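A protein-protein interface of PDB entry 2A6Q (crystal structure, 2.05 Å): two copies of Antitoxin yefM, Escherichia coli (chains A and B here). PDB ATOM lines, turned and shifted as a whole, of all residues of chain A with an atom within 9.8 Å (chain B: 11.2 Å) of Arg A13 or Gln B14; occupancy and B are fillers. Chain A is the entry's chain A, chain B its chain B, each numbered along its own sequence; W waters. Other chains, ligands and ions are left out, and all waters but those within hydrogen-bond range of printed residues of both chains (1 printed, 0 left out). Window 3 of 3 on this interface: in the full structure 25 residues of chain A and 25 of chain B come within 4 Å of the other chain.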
ATOM      1  N   ILE A   7       4.284  -5.529  13.451  1.00  0.00           N
ATOM      2  CA  ILE A   7       4.394  -5.613  14.897  1.00  0.00           C
ATOM      3  C   ILE A   7       5.101  -4.339  15.344  1.00  0.00           C
ATOM      4  O   ILE A   7       5.942  -3.806  14.616  1.00  0.00           O
ATOM      5  CB  ILE A   7       5.211  -6.853  15.321  1.00  0.00           C
ATOM      6  CG1 ILE A   7       5.239  -6.965  16.845  1.00  0.00           C
ATOM      7  CG2 ILE A   7       6.613  -6.771  14.754  1.00  0.00           C
ATOM      8  CD1 ILE A   7       5.851  -8.283  17.354  1.00  0.00           C
ATOM      9  N   SER A   8       4.749  -3.827  16.518  1.00  0.00           N
ATOM     10  CA  SER A   8       5.390  -2.608  17.002  1.00  0.00           C
ATOM     11  C   SER A   8       6.799  -2.902  17.511  1.00  0.00           C
ATOM     12  O   SER A   8       7.126  -4.038  17.857  1.00  0.00           O
ATOM     13  CB  SER A   8       4.573  -1.972  18.129  1.00  0.00           C
ATOM     14  OG  SER A   8       4.505  -2.827  19.256  1.00  0.00           O
ATOM     15  N   TYR A   9       7.635  -1.874  17.538  1.00  0.00           N
ATOM     16  CA  TYR A   9       8.991  -2.041  18.036  1.00  0.00           C
ATOM     17  C   TYR A   9       8.951  -2.662  19.433  1.00  0.00           C
ATOM     18  O   TYR A   9       9.615  -3.663  19.702  1.00  0.00           O
ATOM     19  CB  TYR A   9       9.706  -0.690  18.110  1.00  0.00           C
ATOM     20  CG  TYR A   9      11.021  -0.773  18.852  1.00  0.00           C
ATOM     21  CD1 TYR A   9      12.129  -1.395  18.275  1.00  0.00           C
ATOM     22  CD2 TYR A   9      11.135  -0.310  20.160  1.00  0.00           C
ATOM     23  CE1 TYR A   9      13.317  -1.560  18.984  1.00  0.00           C
ATOM     24  CE2 TYR A   9      12.322  -0.473  20.881  1.00  0.00           C
ATOM     25  CZ  TYR A   9      13.406  -1.102  20.289  1.00  0.00           C
ATOM     26  OH  TYR A   9      14.568  -1.312  21.002  1.00  0.00           O
ATOM     27  N   SER A  10       8.154  -2.062  20.312  1.00  0.00           N
ATOM     28  CA  SER A  10       8.041  -2.523  21.688  1.00  0.00           C
ATOM     29  C   SER A  10       7.575  -3.967  21.856  1.00  0.00           C
ATOM     30  O   SER A  10       8.114  -4.693  22.687  1.00  0.00           O
ATOM     31  CB  SER A  10       7.124  -1.589  22.485  1.00  0.00           C
ATOM     32  OG  SER A  10       7.732  -0.317  22.653  1.00  0.00           O
ATOM     33  N   GLU A  11       6.581  -4.391  21.081  1.00  0.00           N
ATOM     34  CA  GLU A  11       6.112  -5.764  21.212  1.00  0.00           C
ATOM     35  C   GLU A  11       7.185  -6.723  20.721  1.00  0.00           C
ATOM     36  O   GLU A  11       7.403  -7.770  21.320  1.00  0.00           O
ATOM     37  CB  GLU A  11       4.825  -5.990  20.416  1.00  0.00           C
ATOM     38  CG  GLU A  11       4.051  -7.221  20.884  1.00  0.00           C
ATOM     39  CD  GLU A  11       2.844  -7.535  20.015  1.00  0.00           C
ATOM     40  OE1 GLU A  11       2.103  -6.592  19.660  1.00  0.00           O
ATOM     41  OE2 GLU A  11       2.632  -8.729  19.701  1.00  0.00           O
ATOM     42  N   ALA A  12       7.852  -6.361  19.626  1.00  0.00           N
ATOM     43  CA  ALA A  12       8.902  -7.214  19.068  1.00  0.00           C
ATOM     44  C   ALA A  12      10.071  -7.323  20.038  1.00  0.00           C
ATOM     45  O   ALA A  12      10.595  -8.412  20.277  1.00  0.00           O
ATOM     46  CB  ALA A  12       9.387  -6.657  17.730  1.00  0.00           C
ATOM     47  N   ARG A  13      10.478  -6.188  20.592  1.00  0.00           N
ATOM     48  CA  ARG A  13      11.584  -6.173  21.535  1.00  0.00           C
ATOM     49  C   ARG A  13      11.234  -6.952  22.807  1.00  0.00           C
ATOM     50  O   ARG A  13      12.051  -7.713  23.330  1.00  0.00           O
ATOM     51  CB  ARG A  13      11.955  -4.724  21.874  1.00  0.00           C
ATOM     52  CG  ARG A  13      13.163  -4.592  22.798  1.00  0.00           C
ATOM     53  CD  ARG A  13      12.719  -4.330  24.225  1.00  0.00           C
ATOM     54  NE  ARG A  13      13.844  -4.229  25.153  1.00  0.00           N
ATOM     55  CZ  ARG A  13      14.410  -5.265  25.765  1.00  0.00           C
ATOM     56  NH1 ARG A  13      13.959  -6.497  25.548  1.00  0.00           N
ATOM     57  NH2 ARG A  13      15.416  -5.068  26.614  1.00  0.00           N
ATOM     58  N   GLN A  14      10.021  -6.774  23.311  1.00  0.00           N
ATOM     59  CA  GLN A  14       9.641  -7.499  24.506  1.00  0.00           C
ATOM     60  C   GLN A  14       9.516  -9.000  24.225  1.00  0.00           C
ATOM     61  O   GLN A  14       9.758  -9.821  25.106  1.00  0.00           O
ATOM     62  CB  GLN A  14       8.320  -6.961  25.063  1.00  0.00           C
ATOM     63  CG  GLN A  14       7.836  -7.715  26.304  1.00  0.00           C
ATOM     64  CD  GLN A  14       6.686  -7.022  27.013  1.00  0.00           C
ATOM     65  OE1 GLN A  14       6.082  -6.094  26.479  1.00  0.00           O
ATOM     66  NE2 GLN A  14       6.379  -7.474  28.228  1.00  0.00           N
ATOM     67  N   ASN A  15       9.152  -9.354  22.995  1.00  0.00           N
ATOM     68  CA  ASN A  15       8.967 -10.761  22.620  1.00  0.00           C
ATOM     69  C   ASN A  15       9.831 -11.162  21.425  1.00  0.00           C
ATOM     70  O   ASN A  15       9.361 -11.843  20.506  1.00  0.00           O
ATOM     71  CB  ASN A  15       7.490 -11.004  22.282  1.00  0.00           C
ATOM     72  CG  ASN A  15       6.560 -10.571  23.401  1.00  0.00           C
ATOM     73  OD1 ASN A  15       6.503 -11.207  24.449  1.00  0.00           O
ATOM     74  ND2 ASN A  15       5.840  -9.470  23.187  1.00  0.00           N
ATOM     75  N   LEU A  16      11.095 -10.756  21.445  1.00  0.00           N
ATOM     76  CA  LEU A  16      11.991 -11.059  20.337  1.00  0.00           C
ATOM     77  C   LEU A  16      12.112 -12.545  20.045  1.00  0.00           C
ATOM     78  O   LEU A  16      12.021 -12.959  18.896  1.00  0.00           O
ATOM     79  CB  LEU A  16      13.383 -10.471  20.591  1.00  0.00           C
ATOM     80  CG  LEU A  16      14.340 -10.662  19.414  1.00  0.00           C
ATOM     81  CD1 LEU A  16      13.753 -10.020  18.171  1.00  0.00           C
ATOM     82  CD2 LEU A  16      15.690 -10.050  19.746  1.00  0.00           C
ATOM     83  N   SER A  17      12.313 -13.343  21.087  1.00  0.00           N
ATOM     84  CA  SER A  17      12.460 -14.786  20.939  1.00  0.00           C
ATOM     85  C   SER A  17      11.274 -15.406  20.214  1.00  0.00           C
ATOM     86  O   SER A  17      11.441 -16.121  19.232  1.00  0.00           O
ATOM     87  CB  SER A  17      12.607 -15.439  22.315  1.00  0.00           C
ATOM     88  OG  SER A  17      12.703 -16.847  22.193  1.00  0.00           O
ATOM     89  N   ALA A  18      10.077 -15.131  20.713  1.00  0.00           N
ATOM     90  CA  ALA A  18       8.859 -15.657  20.113  1.00  0.00           C
ATOM     91  C   ALA A  18       8.698 -15.166  18.676  1.00  0.00           C
ATOM     92  O   ALA A  18       8.282 -15.922  17.795  1.00  0.00           O
ATOM     93  CB  ALA A  18       7.645 -15.246  20.952  1.00  0.00           C
ATOM     94  N   THR A  19       9.027 -13.898  18.442  1.00  0.00           N
ATOM     95  CA  THR A  19       8.906 -13.314  17.108  1.00  0.00           C
ATOM     96  C   THR A  19       9.812 -14.018  16.102  1.00  0.00           C
ATOM     97  O   THR A  19       9.402 -14.315  14.975  1.00  0.00           O
ATOM     98  CB  THR A  19       9.238 -11.802  17.141  1.00  0.00           C
ATOM     99  OG1 THR A  19       8.284 -11.133  17.976  1.00  0.00           O
ATOM    100  CG2 THR A  19       9.195 -11.199  15.734  1.00  0.00           C
ATOM    101  N   MET A  20      11.047 -14.284  16.507  1.00  0.00           N
ATOM    102  CA  MET A  20      11.992 -14.964  15.634  1.00  0.00           C
ATOM    103  C   MET A  20      11.540 -16.398  15.387  1.00  0.00           C
ATOM    104  O   MET A  20      11.590 -16.883  14.259  1.00  0.00           O
ATOM    105  CB  MET A  20      13.395 -14.970  16.262  1.00  0.00           C
ATOM    106  CG  MET A  20      14.099 -13.619  16.226  1.00  0.00           C
ATOM    107  SD  MET A  20      15.651 -13.651  17.187  1.00  0.00           S
ATOM    108  CE  MET A  20      16.738 -14.587  16.038  1.00  0.00           C
ATOM    109  N   ILE A  30       8.058 -10.481   8.911  1.00  0.00           N
ATOM    110  CA  ILE A  30       7.242  -9.597   9.724  1.00  0.00           C
ATOM    111  C   ILE A  30       7.888  -8.212   9.729  1.00  0.00           C
ATOM    112  O   ILE A  30       9.117  -8.084   9.753  1.00  0.00           O
ATOM    113  CB  ILE A  30       7.044 -10.145  11.164  1.00  0.00           C
ATOM    114  CG1 ILE A  30       5.995  -9.299  11.898  1.00  0.00           C
ATOM    115  CG2 ILE A  30       8.354 -10.139  11.927  1.00  0.00           C
ATOM    116  CD1 ILE A  30       5.517  -9.881  13.236  1.00  0.00           C
ATOM    117  N   ILE A  32       8.683  -4.767  11.517  1.00  0.00           N
ATOM    118  CA  ILE A  32       8.820  -4.121  12.821  1.00  0.00           C
ATOM    119  C   ILE A  32       8.854  -2.621  12.585  1.00  0.00           C
ATOM    120  O   ILE A  32       9.714  -2.127  11.869  1.00  0.00           O
ATOM    121  CB  ILE A  32      10.131  -4.526  13.520  1.00  0.00           C
ATOM    122  CG1 ILE A  32      10.175  -6.046  13.698  1.00  0.00           C
ATOM    123  CG2 ILE A  32      10.233  -3.823  14.870  1.00  0.00           C
ATOM    124  CD1 ILE A  32      11.511  -6.565  14.215  1.00  0.00           C
ATOM    125  N   THR A  33       7.930  -1.895  13.200  1.00  0.00           N
ATOM    126  CA  THR A  33       7.858  -0.454  13.009  1.00  0.00           C
ATOM    127  C   THR A  33       8.078   0.338  14.290  1.00  0.00           C
ATOM    128  O   THR A  33       7.501   0.028  15.327  1.00  0.00           O
ATOM    129  CB  THR A  33       6.486  -0.061  12.470  1.00  0.00           C
ATOM    130  OG1 THR A  33       5.500  -0.311  13.484  1.00  0.00           O
ATOM    131  CG2 THR A  33       6.149  -0.888  11.240  1.00  0.00           C
ATOM    132  N   ARG A  34       8.912   1.368  14.210  1.00  0.00           N
ATOM    133  CA  ARG A  34       9.163   2.223  15.360  1.00  0.00           C
ATOM    134  C   ARG A  34       8.133   3.344  15.279  1.00  0.00           C
ATOM    135  O   ARG A  34       7.720   3.730  14.184  1.00  0.00           O
ATOM    136  CB  ARG A  34      10.573   2.807  15.304  1.00  0.00           C
ATOM    137  CG  ARG A  34      11.678   1.788  15.485  1.00  0.00           C
ATOM    138  CD  ARG A  34      13.034   2.474  15.561  1.00  0.00           C
ATOM    139  NE  ARG A  34      13.092   3.430  16.665  1.00  0.00           N
ATOM    140  CZ  ARG A  34      14.122   4.234  16.911  1.00  0.00           C
ATOM    141  NH1 ARG A  34      15.196   4.205  16.130  1.00  0.00           N
ATOM    142  NH2 ARG A  34      14.081   5.070  17.939  1.00  0.00           N
ATOM    143  N   LEU A  42      11.871  -8.584   9.430  1.00  0.00           N
ATOM    144  CA  LEU A  42      12.604  -9.655  10.083  1.00  0.00           C
ATOM    145  C   LEU A  42      12.130 -10.936   9.407  1.00  0.00           C
ATOM    146  O   LEU A  42      10.925 -11.135   9.231  1.00  0.00           O
ATOM    147  CB  LEU A  42      12.265  -9.721  11.576  1.00  0.00           C
ATOM    148  CG  LEU A  42      12.824 -10.943  12.316  1.00  0.00           C
ATOM    149  CD1 LEU A  42      14.306 -10.731  12.582  1.00  0.00           C
ATOM    150  CD2 LEU A  42      12.084 -11.150  13.626  1.00  0.00           C
ATOM    151  N   MET B   4      29.292  -4.174  11.915  1.00  0.00           N
ATOM    152  CA  MET B   4      28.790  -5.478  12.328  1.00  0.00           C
ATOM    153  C   MET B   4      27.748  -5.988  11.338  1.00  0.00           C
ATOM    154  O   MET B   4      26.949  -5.218  10.804  1.00  0.00           O
ATOM    155  CB  MET B   4      28.164  -5.409  13.727  1.00  0.00           C
ATOM    156  CG  MET B   4      26.853  -4.638  13.794  1.00  0.00           C
ATOM    157  SD  MET B   4      25.881  -4.983  15.284  1.00  0.00           S
ATOM    158  CE  MET B   4      24.772  -6.255  14.682  1.00  0.00           C
ATOM    159  N   ILE B   7      24.858 -10.327  15.152  1.00  0.00           N
ATOM    160  CA  ILE B   7      24.596  -9.994  16.540  1.00  0.00           C
ATOM    161  C   ILE B   7      23.808 -11.152  17.113  1.00  0.00           C
ATOM    162  O   ILE B   7      23.001 -11.772  16.413  1.00  0.00           O
ATOM    163  CB  ILE B   7      23.760  -8.703  16.680  1.00  0.00           C
ATOM    164  CG1 ILE B   7      23.602  -8.354  18.162  1.00  0.00           C
ATOM    165  CG2 ILE B   7      22.377  -8.892  16.049  1.00  0.00           C
ATOM    166  CD1 ILE B   7      23.025  -6.971  18.409  1.00  0.00           C
ATOM    167  N   SER B   8      24.047 -11.460  18.381  1.00  0.00           N
ATOM    168  CA  SER B   8      23.328 -12.549  19.014  1.00  0.00           C
ATOM    169  C   SER B   8      21.946 -12.049  19.417  1.00  0.00           C
ATOM    170  O   SER B   8      21.722 -10.841  19.539  1.00  0.00           O
ATOM    171  CB  SER B   8      24.079 -13.038  20.255  1.00  0.00           C
ATOM    172  OG  SER B   8      24.136 -12.024  21.243  1.00  0.00           O
ATOM    173  N   TYR B   9      21.026 -12.987  19.608  1.00  0.00           N
ATOM    174  CA  TYR B   9      19.668 -12.664  20.022  1.00  0.00           C
ATOM    175  C   TYR B   9      19.746 -11.939  21.368  1.00  0.00           C
ATOM    176  O   TYR B   9      19.141 -10.882  21.561  1.00  0.00           O
ATOM    177  CB  TYR B   9      18.850 -13.955  20.161  1.00  0.00           C
ATOM    178  CG  TYR B   9      17.798 -13.906  21.246  1.00  0.00           C
ATOM    179  CD1 TYR B   9      16.657 -13.111  21.113  1.00  0.00           C
ATOM    180  CD2 TYR B   9      17.969 -14.619  22.433  1.00  0.00           C
ATOM    181  CE1 TYR B   9      15.716 -13.025  22.141  1.00  0.00           C
ATOM    182  CE2 TYR B   9      17.038 -14.540  23.464  1.00  0.00           C
ATOM    183  CZ  TYR B   9      15.913 -13.742  23.317  1.00  0.00           C
ATOM    184  OH  TYR B   9      14.997 -13.661  24.349  1.00  0.00           O
ATOM    185  N   SER B  10      20.511 -12.517  22.292  1.00  0.00           N
ATOM    186  CA  SER B  10      20.675 -11.948  23.623  1.00  0.00           C
ATOM    187  C   SER B  10      21.061 -10.474  23.586  1.00  0.00           C
ATOM    188  O   SER B  10      20.506  -9.662  24.327  1.00  0.00           O
ATOM    189  CB  SER B  10      21.731 -12.731  24.403  1.00  0.00           C
ATOM    190  OG  SER B  10      21.815 -12.257  25.735  1.00  0.00           O
ATOM    191  N   GLU B  11      22.010 -10.126  22.725  1.00  0.00           N
ATOM    192  CA  GLU B  11      22.438  -8.741  22.623  1.00  0.00           C
ATOM    193  C   GLU B  11      21.403  -7.913  21.879  1.00  0.00           C
ATOM    194  O   GLU B  11      21.190  -6.743  22.194  1.00  0.00           O
ATOM    195  CB  GLU B  11      23.787  -8.641  21.908  1.00  0.00           C
ATOM    196  CG  GLU B  11      24.387  -7.240  21.957  1.00  0.00           C
ATOM    197  CD  GLU B  11      25.817  -7.177  21.436  1.00  0.00           C
ATOM    198  OE1 GLU B  11      26.640  -8.028  21.846  1.00  0.00           O
ATOM    199  OE2 GLU B  11      26.119  -6.267  20.630  1.00  0.00           O
ATOM    200  N   ALA B  12      20.755  -8.528  20.893  1.00  0.00           N
ATOM    201  CA  ALA B  12      19.745  -7.845  20.094  1.00  0.00           C
ATOM    202  C   ALA B  12      18.556  -7.377  20.930  1.00  0.00           C
ATOM    203  O   ALA B  12      17.984  -6.324  20.653  1.00  0.00           O
ATOM    204  CB  ALA B  12      19.267  -8.764  18.958  1.00  0.00           C
ATOM    205  N   ARG B  13      18.183  -8.161  21.939  1.00  0.00           N
ATOM    206  CA  ARG B  13      17.060  -7.822  22.822  1.00  0.00           C
ATOM    207  C   ARG B  13      17.168  -6.390  23.316  1.00  0.00           C
ATOM    208  O   ARG B  13      16.205  -5.625  23.280  1.00  0.00           O
ATOM    209  CB  ARG B  13      17.042  -8.699  24.080  1.00  0.00           C
ATOM    210  CG  ARG B  13      16.647 -10.140  23.918  1.00  0.00           C
ATOM    211  CD  ARG B  13      16.608 -10.794  25.290  1.00  0.00           C
ATOM    212  NE  ARG B  13      17.897 -10.673  25.973  1.00  0.00           N
ATOM    213  CZ  ARG B  13      18.133 -11.073  27.220  1.00  0.00           C
ATOM    214  NH1 ARG B  13      17.166 -11.625  27.938  1.00  0.00           N
ATOM    215  NH2 ARG B  13      19.343 -10.934  27.746  1.00  0.00           N
ATOM    216  N   GLN B  14      18.363  -6.056  23.796  1.00  0.00           N
ATOM    217  CA  GLN B  14      18.642  -4.752  24.374  1.00  0.00           C
ATOM    218  C   GLN B  14      19.180  -3.694  23.427  1.00  0.00           C
ATOM    219  O   GLN B  14      19.295  -2.530  23.801  1.00  0.00           O
ATOM    220  CB  GLN B  14      19.594  -4.945  25.554  1.00  0.00           C
ATOM    221  CG  GLN B  14      18.910  -5.614  26.749  1.00  0.00           C
ATOM    222  CD  GLN B  14      19.882  -6.251  27.734  1.00  0.00           C
ATOM    223  OE1 GLN B  14      21.055  -5.878  27.800  1.00  0.00           O
ATOM    224  NE2 GLN B  14      19.388  -7.208  28.515  1.00  0.00           N
ATOM    225  N   ASN B  15      19.497  -4.084  22.198  1.00  0.00           N
ATOM    226  CA  ASN B  15      20.016  -3.126  21.226  1.00  0.00           C
ATOM    227  C   ASN B  15      19.254  -3.177  19.904  1.00  0.00           C
ATOM    228  O   ASN B  15      19.778  -2.791  18.861  1.00  0.00           O
ATOM    229  CB  ASN B  15      21.501  -3.394  20.982  1.00  0.00           C
ATOM    230  CG  ASN B  15      22.354  -3.081  22.198  1.00  0.00           C
ATOM    231  OD1 ASN B  15      22.544  -1.917  22.553  1.00  0.00           O
ATOM    232  ND2 ASN B  15      22.865  -4.121  22.849  1.00  0.00           N
ATOM    233  N   LEU B  16      18.011  -3.640  19.955  1.00  0.00           N
ATOM    234  CA  LEU B  16      17.200  -3.760  18.747  1.00  0.00           C
ATOM    235  C   LEU B  16      17.089  -2.481  17.920  1.00  0.00           C
ATOM    236  O   LEU B  16      17.280  -2.508  16.709  1.00  0.00           O
ATOM    237  CB  LEU B  16      15.795  -4.257  19.096  1.00  0.00           C
ATOM    238  CG  LEU B  16      14.905  -4.485  17.871  1.00  0.00           C
ATOM    239  CD1 LEU B  16      15.556  -5.512  16.951  1.00  0.00           C
ATOM    240  CD2 LEU B  16      13.533  -4.953  18.315  1.00  0.00           C
ATOM    241  N   SER B  17      16.771  -1.369  18.571  1.00  0.00           N
ATOM    242  CA  SER B  17      16.626  -0.089  17.880  1.00  0.00           C
ATOM    243  C   SER B  17      17.894   0.308  17.117  1.00  0.00           C
ATOM    244  O   SER B  17      17.849   0.683  15.940  1.00  0.00           O
ATOM    245  CB  SER B  17      16.276   0.999  18.894  1.00  0.00           C
ATOM    246  OG  SER B  17      16.100   2.246  18.246  1.00  0.00           O
ATOM    247  N   ALA B  18      19.028   0.238  17.803  1.00  0.00           N
ATOM    248  CA  ALA B  18      20.302   0.578  17.186  1.00  0.00           C
ATOM    249  C   ALA B  18      20.551  -0.381  16.026  1.00  0.00           C
ATOM    250  O   ALA B  18      21.004   0.021  14.963  1.00  0.00           O
ATOM    251  CB  ALA B  18      21.431   0.469  18.217  1.00  0.00           C
ATOM    252  N   THR B  19      20.241  -1.655  16.236  1.00  0.00           N
ATOM    253  CA  THR B  19      20.446  -2.664  15.203  1.00  0.00           C
ATOM    254  C   THR B  19      19.610  -2.371  13.959  1.00  0.00           C
ATOM    255  O   THR B  19      20.086  -2.522  12.827  1.00  0.00           O
ATOM    256  CB  THR B  19      20.110  -4.056  15.743  1.00  0.00           C
ATOM    257  OG1 THR B  19      20.901  -4.303  16.909  1.00  0.00           O
ATOM    258  CG2 THR B  19      20.407  -5.132  14.700  1.00  0.00           C
ATOM    259  N   MET B  20      18.366  -1.949  14.168  1.00  0.00           N
ATOM    260  CA  MET B  20      17.491  -1.613  13.056  1.00  0.00           C
ATOM    261  C   MET B  20      18.074  -0.427  12.295  1.00  0.00           C
ATOM    262  O   MET B  20      18.096  -0.416  11.066  1.00  0.00           O
ATOM    263  CB  MET B  20      16.093  -1.255  13.564  1.00  0.00           C
ATOM    264  CG  MET B  20      15.287  -2.448  14.060  1.00  0.00           C
ATOM    265  SD  MET B  20      13.745  -1.943  14.830  1.00  0.00           S
ATOM    266  CE  MET B  20      12.770  -1.498  13.391  1.00  0.00           C
ATOM    267  N   MET B  21      18.539   0.574  13.031  1.00  0.00           N
ATOM    268  CA  MET B  21      19.118   1.756  12.408  1.00  0.00           C
ATOM    269  C   MET B  21      20.343   1.399  11.566  1.00  0.00           C
ATOM    270  O   MET B  21      20.565   1.975  10.508  1.00  0.00           O
ATOM    271  CB  MET B  21      19.502   2.788  13.479  1.00  0.00           C
ATOM    272  CG  MET B  21      18.316   3.306  14.298  1.00  0.00           C
ATOM    273  SD  MET B  21      18.730   4.642  15.469  1.00  0.00           S
ATOM    274  CE  MET B  21      18.973   3.724  17.009  1.00  0.00           C
ATOM    275  N   ILE B  32      20.791 -12.139  12.963  1.00  0.00           N
ATOM    276  CA  ILE B  32      20.608 -12.290  14.395  1.00  0.00           C
ATOM    277  C   ILE B  32      20.722 -13.778  14.694  1.00  0.00           C
ATOM    278  O   ILE B  32      19.821 -14.556  14.395  1.00  0.00           O
ATOM    279  CB  ILE B  32      19.231 -11.787  14.866  1.00  0.00           C
ATOM    280  CG1 ILE B  32      19.061 -10.311  14.506  1.00  0.00           C
ATOM    281  CG2 ILE B  32      19.109 -11.992  16.377  1.00  0.00           C
ATOM    282  CD1 ILE B  32      17.699  -9.721  14.899  1.00  0.00           C
ATOM    283  N   ARG B  34      21.133 -17.327  16.970  1.00  0.00           N
ATOM    284  CA  ARG B  34      20.466 -17.915  18.125  1.00  0.00           C
ATOM    285  C   ARG B  34      21.229 -19.136  18.624  1.00  0.00           C
ATOM    286  O   ARG B  34      21.368 -20.124  17.902  1.00  0.00           O
ATOM    287  CB  ARG B  34      19.036 -18.327  17.771  1.00  0.00           C
ATOM    288  CG  ARG B  34      17.974 -17.409  18.337  1.00  0.00           C
ATOM    289  CD  ARG B  34      16.591 -18.029  18.230  1.00  0.00           C
ATOM    290  NE  ARG B  34      15.652 -17.372  19.133  1.00  0.00           N
ATOM    291  CZ  ARG B  34      15.837 -17.265  20.446  1.00  0.00           C
ATOM    292  NH1 ARG B  34      16.923 -17.771  21.018  1.00  0.00           N
ATOM    293  NH2 ARG B  34      14.944 -16.638  21.190  1.00  0.00           N
ATOM    294  N   LEU B  42      17.517  -9.279   9.632  1.00  0.00           N
ATOM    295  CA  LEU B  42      16.822  -8.008   9.758  1.00  0.00           C
ATOM    296  C   LEU B  42      17.335  -7.123   8.627  1.00  0.00           C
ATOM    297  O   LEU B  42      18.549  -7.038   8.396  1.00  0.00           O
ATOM    298  CB  LEU B  42      17.141  -7.350  11.106  1.00  0.00           C
ATOM    299  CG  LEU B  42      16.318  -6.116  11.483  1.00  0.00           C
ATOM    300  CD1 LEU B  42      14.880  -6.540  11.787  1.00  0.00           C
ATOM    301  CD2 LEU B  42      16.928  -5.432  12.703  1.00  0.00           C
HETATM  302  O   HOH W   1      12.702 -12.660  23.822  1.00  0.00           O
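Printed residues of chain B that touch a printed residue of chain A: Tyr B9, Ala B12, Arg B13, Gln B14, Leu B16, Ser B17, Met B20, Met B21, Ile B32 and Arg B34.
Hydrophobic or aromatic side chains of chain B that line the printed part of chain A: Tyr B9, Ala B12, Leu B16, Met B20, Met B21 and Ile B32.
Of the 19 printed residues of chain A, 7 touch a printed residue of chain B.
Among the printed residues, no Asp or Glu carboxylate lies within 4 Å of a Lys or Arg side-chain nitrogen of the other chain.
O of Ser B10 is in hydrogen-bond range of NE of Arg B13 (3.2 Å).
N of Tyr A9 lies within hydrogen-bond range of O of Thr A33.
Water W1 lies within hydrogen-bond range of the side-chain hydroxyl of Tyr B9, the backbone NH of Ser A17 and the backbone NH of Leu A16.
Arg B13 touches its own counterpart, Arg A13.
Arg A13 touches Gln B14, but with the chains exchanged Gln A14 does not touch Arg B13 (6.3 Å).
Arg A13 touches Leu B16, and with the chains exchanged Leu A16 touches Arg B13.
Leu A16 touches Ala B12, but with the chains exchanged Ala A12 does not touch Leu B16 (4.5 Å).
17 positions are printed for both chains.
Of the printed residues of chain B, Tyr A9 touches Leu B16, Ser B17 and Met B20.
No residue of chain B comes within 4 Å of Ser A10.
Arg A13 touches three residues of chain B.
Of the printed residues of chain B, Leu A16 touches Tyr B9, Ala B12 and Arg B13.
Ala A18 touches none of the printed residues of chain B.
Of the printed residues of chain B, Ile A32 touches Met B20 (3.5 Å).
Ala B12 touches just one residue of chain A: Leu A16.
Arg B13 touches just these residues of chain A: Arg A13 (3.1 Å) and Leu A16 (3.8 Å).
Gln B14 touches just one residue of chain A: Arg A13.
No residue of chain A comes within 4 Å of Asn B15.
Of the printed residues of chain A, Leu B16 touches Tyr A9 and Arg A13.
Of the printed residues of chain A, Ser B17 touches Tyr A9 (3.3 Å) and Arg A34 (3.0 Å).
Of the printed residues of chain A, Ile B32 touches Met A20 (3.5 Å).
Of the printed residues of chain A, Arg B34 touches Ser A17 and Met A20.
Leu B42 touches none of the printed residues of chain A.
Among the printed residues, merely in contact across the chains: Tyr A9 with Leu B16, Tyr A9 with Met B20, Arg A13 with Gln B14, Arg A13 with Leu B16, Leu A16 with Tyr B9, Leu A16 with Ala B12, Leu A16 with Arg B13, Ser A17 with Tyr B9, Met A20 with Ile B32, Met A20 with Arg B34 and Ile A32 with Met B20.
NH1 of Arg A13 sits close to O of Arg B13 (3.3 Å).
The side-chain sulfur (SD) of Met B21 lies within hydrogen-bond range of the guanidinium group (NH1) of Arg A34.
NH2 of Arg B34 lies within hydrogen-bond range of OG of Ser A17 (2.5 Å).
The side-chain hydroxyl (OH) of Tyr A9 is in hydrogen-bond range of the backbone NH (N) of Ser B17, at 3.3 Å.
The side-chain hydroxyl (OG) of Ser B17 lies within hydrogen-bond range of the guanidinium group (NH1) of Arg A34.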
